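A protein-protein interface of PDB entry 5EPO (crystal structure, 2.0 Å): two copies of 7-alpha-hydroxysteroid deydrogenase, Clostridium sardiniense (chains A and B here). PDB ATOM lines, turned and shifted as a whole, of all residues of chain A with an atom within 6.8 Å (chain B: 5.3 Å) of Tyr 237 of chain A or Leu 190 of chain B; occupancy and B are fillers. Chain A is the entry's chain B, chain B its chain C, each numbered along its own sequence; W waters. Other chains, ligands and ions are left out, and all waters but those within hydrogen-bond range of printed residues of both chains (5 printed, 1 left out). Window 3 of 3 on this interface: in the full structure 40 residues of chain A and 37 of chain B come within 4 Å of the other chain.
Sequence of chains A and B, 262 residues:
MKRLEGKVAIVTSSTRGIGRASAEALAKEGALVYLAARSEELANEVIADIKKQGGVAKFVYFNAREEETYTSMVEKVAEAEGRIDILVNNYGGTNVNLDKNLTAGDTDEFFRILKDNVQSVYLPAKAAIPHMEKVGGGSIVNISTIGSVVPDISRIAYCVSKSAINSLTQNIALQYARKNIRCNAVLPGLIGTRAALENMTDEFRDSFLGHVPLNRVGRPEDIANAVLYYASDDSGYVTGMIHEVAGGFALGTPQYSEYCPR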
ATOM      1  N   ARG A 182      18.519  -9.213  24.798  1.00  0.00           N
ATOM      2  CA  ARG A 182      17.208  -8.819  25.295  1.00  0.00           C
ATOM      3  C   ARG A 182      16.778  -9.719  26.418  1.00  0.00           C
ATOM      4  O   ARG A 182      17.154 -10.888  26.467  1.00  0.00           O
ATOM      5  CB  ARG A 182      16.180  -8.838  24.144  1.00  0.00           C
ATOM      6  CG  ARG A 182      16.472  -7.784  23.080  1.00  0.00           C
ATOM      7  CD  ARG A 182      15.579  -7.827  21.854  1.00  0.00           C
ATOM      8  NE  ARG A 182      15.553  -9.134  21.207  1.00  0.00           N
ATOM      9  CZ  ARG A 182      14.578 -10.016  21.305  1.00  0.00           C
ATOM     10  NH1 ARG A 182      13.476  -9.780  22.055  1.00  0.00           N
ATOM     11  NH2 ARG A 182      14.695 -11.168  20.671  1.00  0.00           N
ATOM     12  N   SER A 232      12.702 -14.853  19.242  1.00  0.00           N
ATOM     13  CA  SER A 232      13.027 -14.600  17.857  1.00  0.00           C
ATOM     14  C   SER A 232      13.178 -13.118  17.551  1.00  0.00           C
ATOM     15  O   SER A 232      12.823 -12.269  18.345  1.00  0.00           O
ATOM     16  CB  SER A 232      11.956 -15.190  16.956  1.00  0.00           C
ATOM     17  OG  SER A 232      10.763 -14.435  17.013  1.00  0.00           O
ATOM     18  N   ASP A 233      13.703 -12.828  16.366  1.00  0.00           N
ATOM     19  CA  ASP A 233      13.900 -11.463  15.934  1.00  0.00           C
ATOM     20  C   ASP A 233      12.572 -10.748  15.644  1.00  0.00           C
ATOM     21  O   ASP A 233      12.548  -9.521  15.421  1.00  0.00           O
ATOM     22  CB  ASP A 233      14.765 -11.420  14.676  1.00  0.00           C
ATOM     23  CG  ASP A 233      16.213 -11.236  14.984  1.00  0.00           C
ATOM     24  OD1 ASP A 233      16.586 -10.135  15.489  1.00  0.00           O
ATOM     25  OD2 ASP A 233      16.968 -12.197  14.684  1.00  0.00           O
ATOM     26  N   ASP A 234      11.485 -11.491  15.621  1.00  0.00           N
ATOM     27  CA  ASP A 234      10.167 -10.858  15.531  1.00  0.00           C
ATOM     28  C   ASP A 234       9.900  -9.897  16.698  1.00  0.00           C
ATOM     29  O   ASP A 234       9.035  -9.033  16.586  1.00  0.00           O
ATOM     30  CB  ASP A 234       9.034 -11.892  15.472  1.00  0.00           C
ATOM     31  CG  ASP A 234       8.836 -12.461  14.071  1.00  0.00           C
ATOM     32  OD1 ASP A 234       9.768 -12.344  13.207  1.00  0.00           O
ATOM     33  OD2 ASP A 234       7.745 -13.047  13.843  1.00  0.00           O
ATOM     34  N   SER A 235      10.656 -10.048  17.785  1.00  0.00           N
ATOM     35  CA  SER A 235      10.568  -9.150  18.933  1.00  0.00           C
ATOM     36  C   SER A 235      11.910  -8.429  19.148  1.00  0.00           C
ATOM     37  O   SER A 235      12.248  -8.027  20.263  1.00  0.00           O
ATOM     38  CB  SER A 235      10.214  -9.936  20.193  1.00  0.00           C
ATOM     39  OG  SER A 235      11.295 -10.812  20.529  1.00  0.00           O
ATOM     40  N   GLY A 236      12.639  -8.248  18.063  1.00  0.00           N
ATOM     41  CA  GLY A 236      13.982  -7.692  18.134  1.00  0.00           C
ATOM     42  C   GLY A 236      14.073  -6.287  18.688  1.00  0.00           C
ATOM     43  O   GLY A 236      15.147  -5.856  19.078  1.00  0.00           O
ATOM     44  N   TYR A 237      12.968  -5.565  18.716  1.00  0.00           N
ATOM     45  CA  TYR A 237      12.978  -4.213  19.248  1.00  0.00           C
ATOM     46  C   TYR A 237      12.226  -4.167  20.596  1.00  0.00           C
ATOM     47  O   TYR A 237      11.809  -3.095  21.065  1.00  0.00           O
ATOM     48  CB  TYR A 237      12.322  -3.257  18.237  1.00  0.00           C
ATOM     49  CG  TYR A 237      12.780  -1.824  18.342  1.00  0.00           C
ATOM     50  CD1 TYR A 237      14.085  -1.491  18.423  1.00  0.00           C
ATOM     51  CD2 TYR A 237      11.840  -0.790  18.304  1.00  0.00           C
ATOM     52  CE1 TYR A 237      14.498  -0.164  18.466  1.00  0.00           C
ATOM     53  CE2 TYR A 237      12.249   0.553  18.340  1.00  0.00           C
ATOM     54  CZ  TYR A 237      13.592   0.844  18.430  1.00  0.00           C
ATOM     55  OH  TYR A 237      13.996   2.181  18.456  1.00  0.00           O
ATOM     56  N   VAL A 238      12.078  -5.327  21.209  1.00  0.00           N
ATOM     57  CA  VAL A 238      11.303  -5.455  22.444  1.00  0.00           C
ATOM     58  C   VAL A 238      12.149  -6.030  23.581  1.00  0.00           C
ATOM     59  O   VAL A 238      12.674  -7.139  23.483  1.00  0.00           O
ATOM     60  CB  VAL A 238      10.072  -6.325  22.218  1.00  0.00           C
ATOM     61  CG1 VAL A 238       9.210  -6.417  23.466  1.00  0.00           C
ATOM     62  CG2 VAL A 238       9.253  -5.827  21.029  1.00  0.00           C
ATOM     63  N   THR A 239      12.235  -5.284  24.663  1.00  0.00           N
ATOM     64  CA  THR A 239      13.040  -5.729  25.794  1.00  0.00           C
ATOM     65  C   THR A 239      12.451  -5.141  27.077  1.00  0.00           C
ATOM     66  O   THR A 239      11.922  -4.037  27.092  1.00  0.00           O
ATOM     67  CB  THR A 239      14.511  -5.379  25.599  1.00  0.00           C
ATOM     68  OG1 THR A 239      15.321  -6.147  26.498  1.00  0.00           O
ATOM     69  CG2 THR A 239      14.780  -3.886  25.778  1.00  0.00           C
ATOM     70  N   PRO B 188       4.451   1.787  19.696  1.00  0.00           N
ATOM     71  CA  PRO B 188       5.755   1.966  19.045  1.00  0.00           C
ATOM     72  C   PRO B 188       6.561   3.096  19.634  1.00  0.00           C
ATOM     73  O   PRO B 188       5.991   4.066  20.103  1.00  0.00           O
ATOM     74  CB  PRO B 188       5.396   2.322  17.599  1.00  0.00           C
ATOM     75  CG  PRO B 188       3.925   2.095  17.478  1.00  0.00           C
ATOM     76  CD  PRO B 188       3.347   2.272  18.858  1.00  0.00           C
ATOM     77  N   GLY B 189       7.890   2.952  19.640  1.00  0.00           N
ATOM     78  CA  GLY B 189       8.750   4.078  19.880  1.00  0.00           C
ATOM     79  C   GLY B 189       9.099   4.737  18.571  1.00  0.00           C
ATOM     80  O   GLY B 189       8.252   4.817  17.665  1.00  0.00           O
ATOM     81  N   LEU B 190      10.362   5.180  18.440  1.00  0.00           N
ATOM     82  CA  LEU B 190      10.772   5.892  17.241  1.00  0.00           C
ATOM     83  C   LEU B 190      10.937   4.938  16.094  1.00  0.00           C
ATOM     84  O   LEU B 190      11.850   4.098  16.107  1.00  0.00           O
ATOM     85  CB  LEU B 190      12.085   6.631  17.487  1.00  0.00           C
ATOM     86  CG  LEU B 190      12.698   7.312  16.241  1.00  0.00           C
ATOM     87  CD1 LEU B 190      11.755   8.357  15.697  1.00  0.00           C
ATOM     88  CD2 LEU B 190      14.002   7.956  16.654  1.00  0.00           C
ATOM     89  N   ILE B 191      10.054   5.048  15.103  1.00  0.00           N
ATOM     90  CA  ILE B 191      10.070   4.166  13.925  1.00  0.00           C
ATOM     91  C   ILE B 191      10.400   4.968  12.670  1.00  0.00           C
ATOM     92  O   ILE B 191       9.823   6.032  12.444  1.00  0.00           O
ATOM     93  CB  ILE B 191       8.713   3.473  13.722  1.00  0.00           C
ATOM     94  CG1 ILE B 191       8.255   2.805  15.019  1.00  0.00           C
ATOM     95  CG2 ILE B 191       8.797   2.434  12.617  1.00  0.00           C
ATOM     96  CD1 ILE B 191       9.195   1.772  15.587  1.00  0.00           C
ATOM     97  N   GLY B 192      11.276   4.428  11.838  1.00  0.00           N
ATOM     98  CA  GLY B 192      11.656   5.048  10.579  1.00  0.00           C
ATOM     99  C   GLY B 192      10.590   5.165   9.478  1.00  0.00           C
ATOM    100  O   GLY B 192      10.809   4.735   8.354  1.00  0.00           O
ATOM    101  N   ALA B 196       7.539  10.225  11.608  1.00  0.00           N
ATOM    102  CA  ALA B 196       8.642  10.620  12.475  1.00  0.00           C
ATOM    103  C   ALA B 196       9.724  11.371  11.728  1.00  0.00           C
ATOM    104  O   ALA B 196      10.247  12.371  12.218  1.00  0.00           O
ATOM    105  CB  ALA B 196       9.246   9.415  13.161  1.00  0.00           C
ATOM    106  N   ARG B 205      15.393  13.514  16.878  1.00  0.00           N
ATOM    107  CA  ARG B 205      15.472  12.067  16.663  1.00  0.00           C
ATOM    108  C   ARG B 205      16.835  11.513  17.064  1.00  0.00           C
ATOM    109  O   ARG B 205      16.944  10.379  17.520  1.00  0.00           O
ATOM    110  CB  ARG B 205      15.156  11.719  15.195  1.00  0.00           C
ATOM    111  CG  ARG B 205      13.658  11.830  14.894  1.00  0.00           C
ATOM    112  CD  ARG B 205      13.312  11.458  13.479  1.00  0.00           C
ATOM    113  NE  ARG B 205      13.543  12.580  12.575  1.00  0.00           N
ATOM    114  CZ  ARG B 205      14.648  12.762  11.850  1.00  0.00           C
ATOM    115  NH1 ARG B 205      15.647  11.878  11.883  1.00  0.00           N
ATOM    116  NH2 ARG B 205      14.741  13.839  11.072  1.00  0.00           N
ATOM    117  N   PHE B 208      16.643  11.420  20.820  1.00  0.00           N
ATOM    118  CA  PHE B 208      15.761  10.326  21.206  1.00  0.00           C
ATOM    119  C   PHE B 208      16.507   9.006  21.117  1.00  0.00           C
ATOM    120  O   PHE B 208      16.520   8.235  22.083  1.00  0.00           O
ATOM    121  CB  PHE B 208      14.501  10.329  20.365  1.00  0.00           C
ATOM    122  CG  PHE B 208      13.412   9.399  20.876  1.00  0.00           C
ATOM    123  CD1 PHE B 208      13.446   8.034  20.598  1.00  0.00           C
ATOM    124  CD2 PHE B 208      12.344   9.900  21.618  1.00  0.00           C
ATOM    125  CE1 PHE B 208      12.450   7.196  21.034  1.00  0.00           C
ATOM    126  CE2 PHE B 208      11.335   9.067  22.068  1.00  0.00           C
ATOM    127  CZ  PHE B 208      11.381   7.714  21.778  1.00  0.00           C
ATOM    128  N   LEU B 209      17.181   8.788  19.999  1.00  0.00           N
ATOM    129  CA  LEU B 209      17.921   7.554  19.762  1.00  0.00           C
ATOM    130  C   LEU B 209      18.985   7.282  20.821  1.00  0.00           C
ATOM    131  O   LEU B 209      19.258   6.133  21.141  1.00  0.00           O
ATOM    132  CB  LEU B 209      18.573   7.582  18.370  1.00  0.00           C
ATOM    133  CG  LEU B 209      19.363   6.351  17.954  1.00  0.00           C
ATOM    134  CD1 LEU B 209      18.533   5.100  18.028  1.00  0.00           C
ATOM    135  CD2 LEU B 209      19.895   6.504  16.529  1.00  0.00           C
ATOM    136  N   VAL B 212      17.649   5.167  23.540  1.00  0.00           N
ATOM    137  CA  VAL B 212      17.119   3.862  23.166  1.00  0.00           C
ATOM    138  C   VAL B 212      18.174   2.783  23.455  1.00  0.00           C
ATOM    139  O   VAL B 212      19.199   2.681  22.762  1.00  0.00           O
ATOM    140  CB  VAL B 212      16.718   3.813  21.668  1.00  0.00           C
ATOM    141  CG1 VAL B 212      16.171   2.457  21.273  1.00  0.00           C
ATOM    142  CG2 VAL B 212      15.675   4.884  21.363  1.00  0.00           C
ATOM    143  N   LEU B 214      18.476  -0.404  22.908  1.00  0.00           N
ATOM    144  CA  LEU B 214      18.840  -1.352  21.857  1.00  0.00           C
ATOM    145  C   LEU B 214      19.479  -0.631  20.682  1.00  0.00           C
ATOM    146  O   LEU B 214      19.838  -1.248  19.710  1.00  0.00           O
ATOM    147  CB  LEU B 214      17.623  -2.182  21.429  1.00  0.00           C
ATOM    148  CG  LEU B 214      17.262  -3.262  22.423  1.00  0.00           C
ATOM    149  CD1 LEU B 214      15.876  -3.803  22.099  1.00  0.00           C
ATOM    150  CD2 LEU B 214      18.312  -4.373  22.409  1.00  0.00           C
ATOM    151  N   ARG B 216      19.034   1.504  18.073  1.00  0.00           N
ATOM    152  CA  ARG B 216      18.695   1.694  16.651  1.00  0.00           C
ATOM    153  C   ARG B 216      17.294   2.278  16.587  1.00  0.00           C
ATOM    154  O   ARG B 216      16.548   2.259  17.587  1.00  0.00           O
ATOM    155  CB  ARG B 216      18.730   0.368  15.882  1.00  0.00           C
ATOM    156  CG  ARG B 216      17.693  -0.675  16.309  1.00  0.00           C
ATOM    157  CD  ARG B 216      17.865  -1.966  15.551  1.00  0.00           C
ATOM    158  NE  ARG B 216      16.971  -3.047  15.931  1.00  0.00           N
ATOM    159  CZ  ARG B 216      15.690  -3.158  15.544  1.00  0.00           C
ATOM    160  NH1 ARG B 216      15.113  -2.233  14.768  1.00  0.00           N
ATOM    161  NH2 ARG B 216      14.979  -4.218  15.919  1.00  0.00           N
ATOM    162  N   VAL B 217      16.968   2.827  15.430  1.00  0.00           N
ATOM    163  CA  VAL B 217      15.593   3.252  15.118  1.00  0.00           C
ATOM    164  C   VAL B 217      14.819   1.983  14.771  1.00  0.00           C
ATOM    165  O   VAL B 217      15.357   1.080  14.151  1.00  0.00           O
ATOM    166  CB  VAL B 217      15.581   4.249  13.952  1.00  0.00           C
ATOM    167  CG1 VAL B 217      14.154   4.636  13.560  1.00  0.00           C
ATOM    168  CG2 VAL B 217      16.296   5.522  14.371  1.00  0.00           C
ATOM    169  N   GLY B 218      13.563   1.908  15.175  1.00  0.00           N
ATOM    170  CA  GLY B 218      12.723   0.774  14.846  1.00  0.00           C
ATOM    171  C   GLY B 218      12.273   0.777  13.396  1.00  0.00           C
ATOM    172  O   GLY B 218      12.415   1.780  12.688  1.00  0.00           O
ATOM    173  N   ASP B 222       8.844  -4.155  12.844  1.00  0.00           N
ATOM    174  CA  ASP B 222       8.876  -4.464  14.272  1.00  0.00           C
ATOM    175  C   ASP B 222       7.464  -4.358  14.841  1.00  0.00           C
ATOM    176  O   ASP B 222       7.042  -5.228  15.615  1.00  0.00           O
ATOM    177  CB  ASP B 222       9.811  -3.544  15.033  1.00  0.00           C
ATOM    178  CG  ASP B 222      11.269  -3.705  14.610  1.00  0.00           C
ATOM    179  OD1 ASP B 222      11.724  -4.841  14.527  1.00  0.00           O
ATOM    180  OD2 ASP B 222      11.949  -2.664  14.391  1.00  0.00           O
ATOM    181  N   GLU B 244       5.036  -2.808  24.606  1.00  0.00           N
ATOM    182  CA  GLU B 244       6.003  -1.772  24.226  1.00  0.00           C
ATOM    183  C   GLU B 244       6.978  -2.244  23.159  1.00  0.00           C
ATOM    184  O   GLU B 244       7.668  -3.248  23.333  1.00  0.00           O
ATOM    185  CB  GLU B 244       6.778  -1.342  25.469  1.00  0.00           C
ATOM    186  CG  GLU B 244       5.897  -0.771  26.559  1.00  0.00           C
ATOM    187  CD  GLU B 244       6.664  -0.341  27.786  1.00  0.00           C
ATOM    188  OE1 GLU B 244       7.917  -0.322  27.730  1.00  0.00           O
ATOM    189  OE2 GLU B 244       6.040  -0.011  28.813  1.00  0.00           O
ATOM    190  N   VAL B 245       7.024  -1.526  22.053  1.00  0.00           N
ATOM    191  CA  VAL B 245       7.956  -1.841  20.966  1.00  0.00           C
ATOM    192  C   VAL B 245       8.750  -0.564  20.677  1.00  0.00           C
ATOM    193  O   VAL B 245       8.486   0.122  19.696  1.00  0.00           O
ATOM    194  CB  VAL B 245       7.234  -2.341  19.728  1.00  0.00           C
ATOM    195  CG1 VAL B 245       8.242  -2.865  18.713  1.00  0.00           C
ATOM    196  CG2 VAL B 245       6.300  -3.489  20.080  1.00  0.00           C
ATOM    197  N   ALA B 246       9.691  -0.249  21.565  1.00  0.00           N
ATOM    198  CA  ALA B 246      10.365   1.040  21.548  1.00  0.00           C
ATOM    199  C   ALA B 246      11.853   0.873  21.841  1.00  0.00           C
ATOM    200  O   ALA B 246      12.536   1.828  22.209  1.00  0.00           O
ATOM    201  CB  ALA B 246       9.717   1.984  22.563  1.00  0.00           C
ATOM    202  N   GLY B 247      12.358  -0.342  21.704  1.00  0.00           N
ATOM    203  CA  GLY B 247      13.795  -0.579  21.878  1.00  0.00           C
ATOM    204  C   GLY B 247      14.270  -0.472  23.319  1.00  0.00           C
ATOM    205  O   GLY B 247      15.494  -0.368  23.558  1.00  0.00           O
ATOM    206  N   GLY B 248      13.335  -0.481  24.277  1.00  0.00           N
ATOM    207  CA  GLY B 248      13.670  -0.299  25.678  1.00  0.00           C
ATOM    208  C   GLY B 248      13.626   1.154  26.134  1.00  0.00           C
ATOM    209  O   GLY B 248      13.978   1.451  27.286  1.00  0.00           O
HETATM  210  O   HOH W   1       9.420  -3.123  27.626  1.00  0.00           O
HETATM  211  O   HOH W   2      10.479  -5.970  17.557  1.00  0.00           O
HETATM  212  O   HOH W   3       9.876  -3.469  24.934  1.00  0.00           O
HETATM  213  O   HOH W   4      12.263   3.793  20.033  1.00  0.00           O
HETATM  214  O   HOH W   5       7.719  -6.973  17.679  1.00  0.00           O
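O of Arg 216 of chain B lies within hydrogen-bond range of OH of Tyr 237 of chain A.
N of Gly 218 of chain B sits at hydrogen-bond distance from OH of Tyr 237 of chain A (3.3 Å).
The backbone carbonyl oxygen of Tyr 237 of chain A lies within hydrogen-bond range of the backbone NH of Gly 247 of chain B (2.9 Å).
The guanidinium group (NH2) of Arg 182 of chain A is in hydrogen-bond range of the backbone carbonyl oxygen (O) of Ser 232 of chain A (3.2 Å).
O of Val 238 of chain A sits at hydrogen-bond distance from NH1 of Arg 182 of chain A.
O of Leu 190 of chain B sits at hydrogen-bond distance from N of Gly 218 of chain B (2.9 Å).
The backbone NH of Gly 192 of chain B is in hydrogen-bond range of the backbone carbonyl oxygen of Gly 218 of chain B.
N of Leu 214 of chain B sits at hydrogen-bond distance from O of Gly 247 of chain B (3.1 Å).
The guanidinium group of Arg 216 of chain B is in salt-bridge range of the side-chain carboxylate of Asp 222 of chain B, 3.2 Å away.
Gly 236 of chain A touches Leu 214 of chain B (O to CD1, 3.7 Å).
Gly 236 of chain A touches Arg 216 of chain B (O to NH2, 3.6 Å).
Tyr 237 of chain A touches Leu 190 of chain B.
Leu 214 of chain B touches Tyr 237 of chain A (CD1 to C, 3.96 Å).
OH of Tyr 237 of chain A touches C of Val 217 of chain B, at 3.8 Å.
Asp 222 of chain B touches Tyr 237 of chain A (CG to CB, 3.8 Å).
CD2 of Tyr 237 of chain A touches O of Val 245 of chain B, at 3.7 Å.
O of Glu 244 of chain B touches CG1 of Val 238 of chain A, at 3.5 Å.
Val 245 of chain B touches Val 238 of chain A.
CD1 of Leu 214 of chain B touches CG2 of Thr 239 of chain A (3.8 Å).
Asp 234 of chain A touches none of the printed residues of chain B.
Of the printed residues of chain B, Tyr 237 of chain A touches Leu 190, Val 212, Leu 214, Arg 216, Val 217, Gly 218, Asp 222, Val 245, Ala 246 and Gly 247.
Printed residues of chain B within 4 Å of Thr 239 of chain A: Leu 214 (3.8 Å) and Gly 248 (3.8 Å).
Pro 188 of chain B touches none of the printed residues of chain A.
Of the printed residues of chain A, Leu 190 of chain B touches Tyr 237 (3.7 Å).
Printed residues of chain A within 4 Å of Val 217 of chain B: Tyr 237.
Printed residues of chain A within 4 Å of Glu 244 of chain B: Val 238.
Printed residues of chain A within 4 Å of Val 245 of chain B: Tyr 237 (3.7 Å) and Val 238 (3.9 Å).
The nearest residue of chain B that does not touch Tyr 237 of chain A is Ile 191 of chain B (4.3 Å).
The nearest printed residue of chain A that does not touch Leu 190 of chain B is Val 238 of chain A (10.7 Å).
Of the 9 printed residues of chain A, 5 touch a printed residue of chain B.
Hydrophobic or aromatic side chains of chain A that line the printed part of chain B: Tyr 237 and Val 238.
Of the 20 printed residues of chain B, 12 touch a printed residue of chain A.
Hydrophobic or aromatic side chains of chain B that line the printed part of chain A: Val 212, Leu 214 and Val 245.
Among the printed residues, no Asp or Glu carboxylate lies within 4 Å of a Lys or Arg side-chain nitrogen of the other chain.
No position is printed for both chains.
Of the 17 pairs that touch across the chains among the printed residues, none has its exchanged pair printed and touching as well.
Water W5 bridges O of Asp 234 of chain A (2.7 Å) and O of Asp 222 of chain B (2.8 Å).
Water W1 lies within hydrogen-bond range of O of Thr 239 of chain A and OE1 of Glu 244 of chain B.
Water W3 bridges O of Glu 244 of chain B and N of Thr 239 of chain A.
Water W2 lies within hydrogen-bond range of N of Tyr 237 of chain A (2.8 Å), N of Gly 236 of chain A (3.2 Å) and OD1 of Asp 222 of chain B (3.5 Å).
Water W4 lies within hydrogen-bond range of N of Leu 190 of chain B, OH of Tyr 237 of chain A and O of Ala 246 of chain B.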
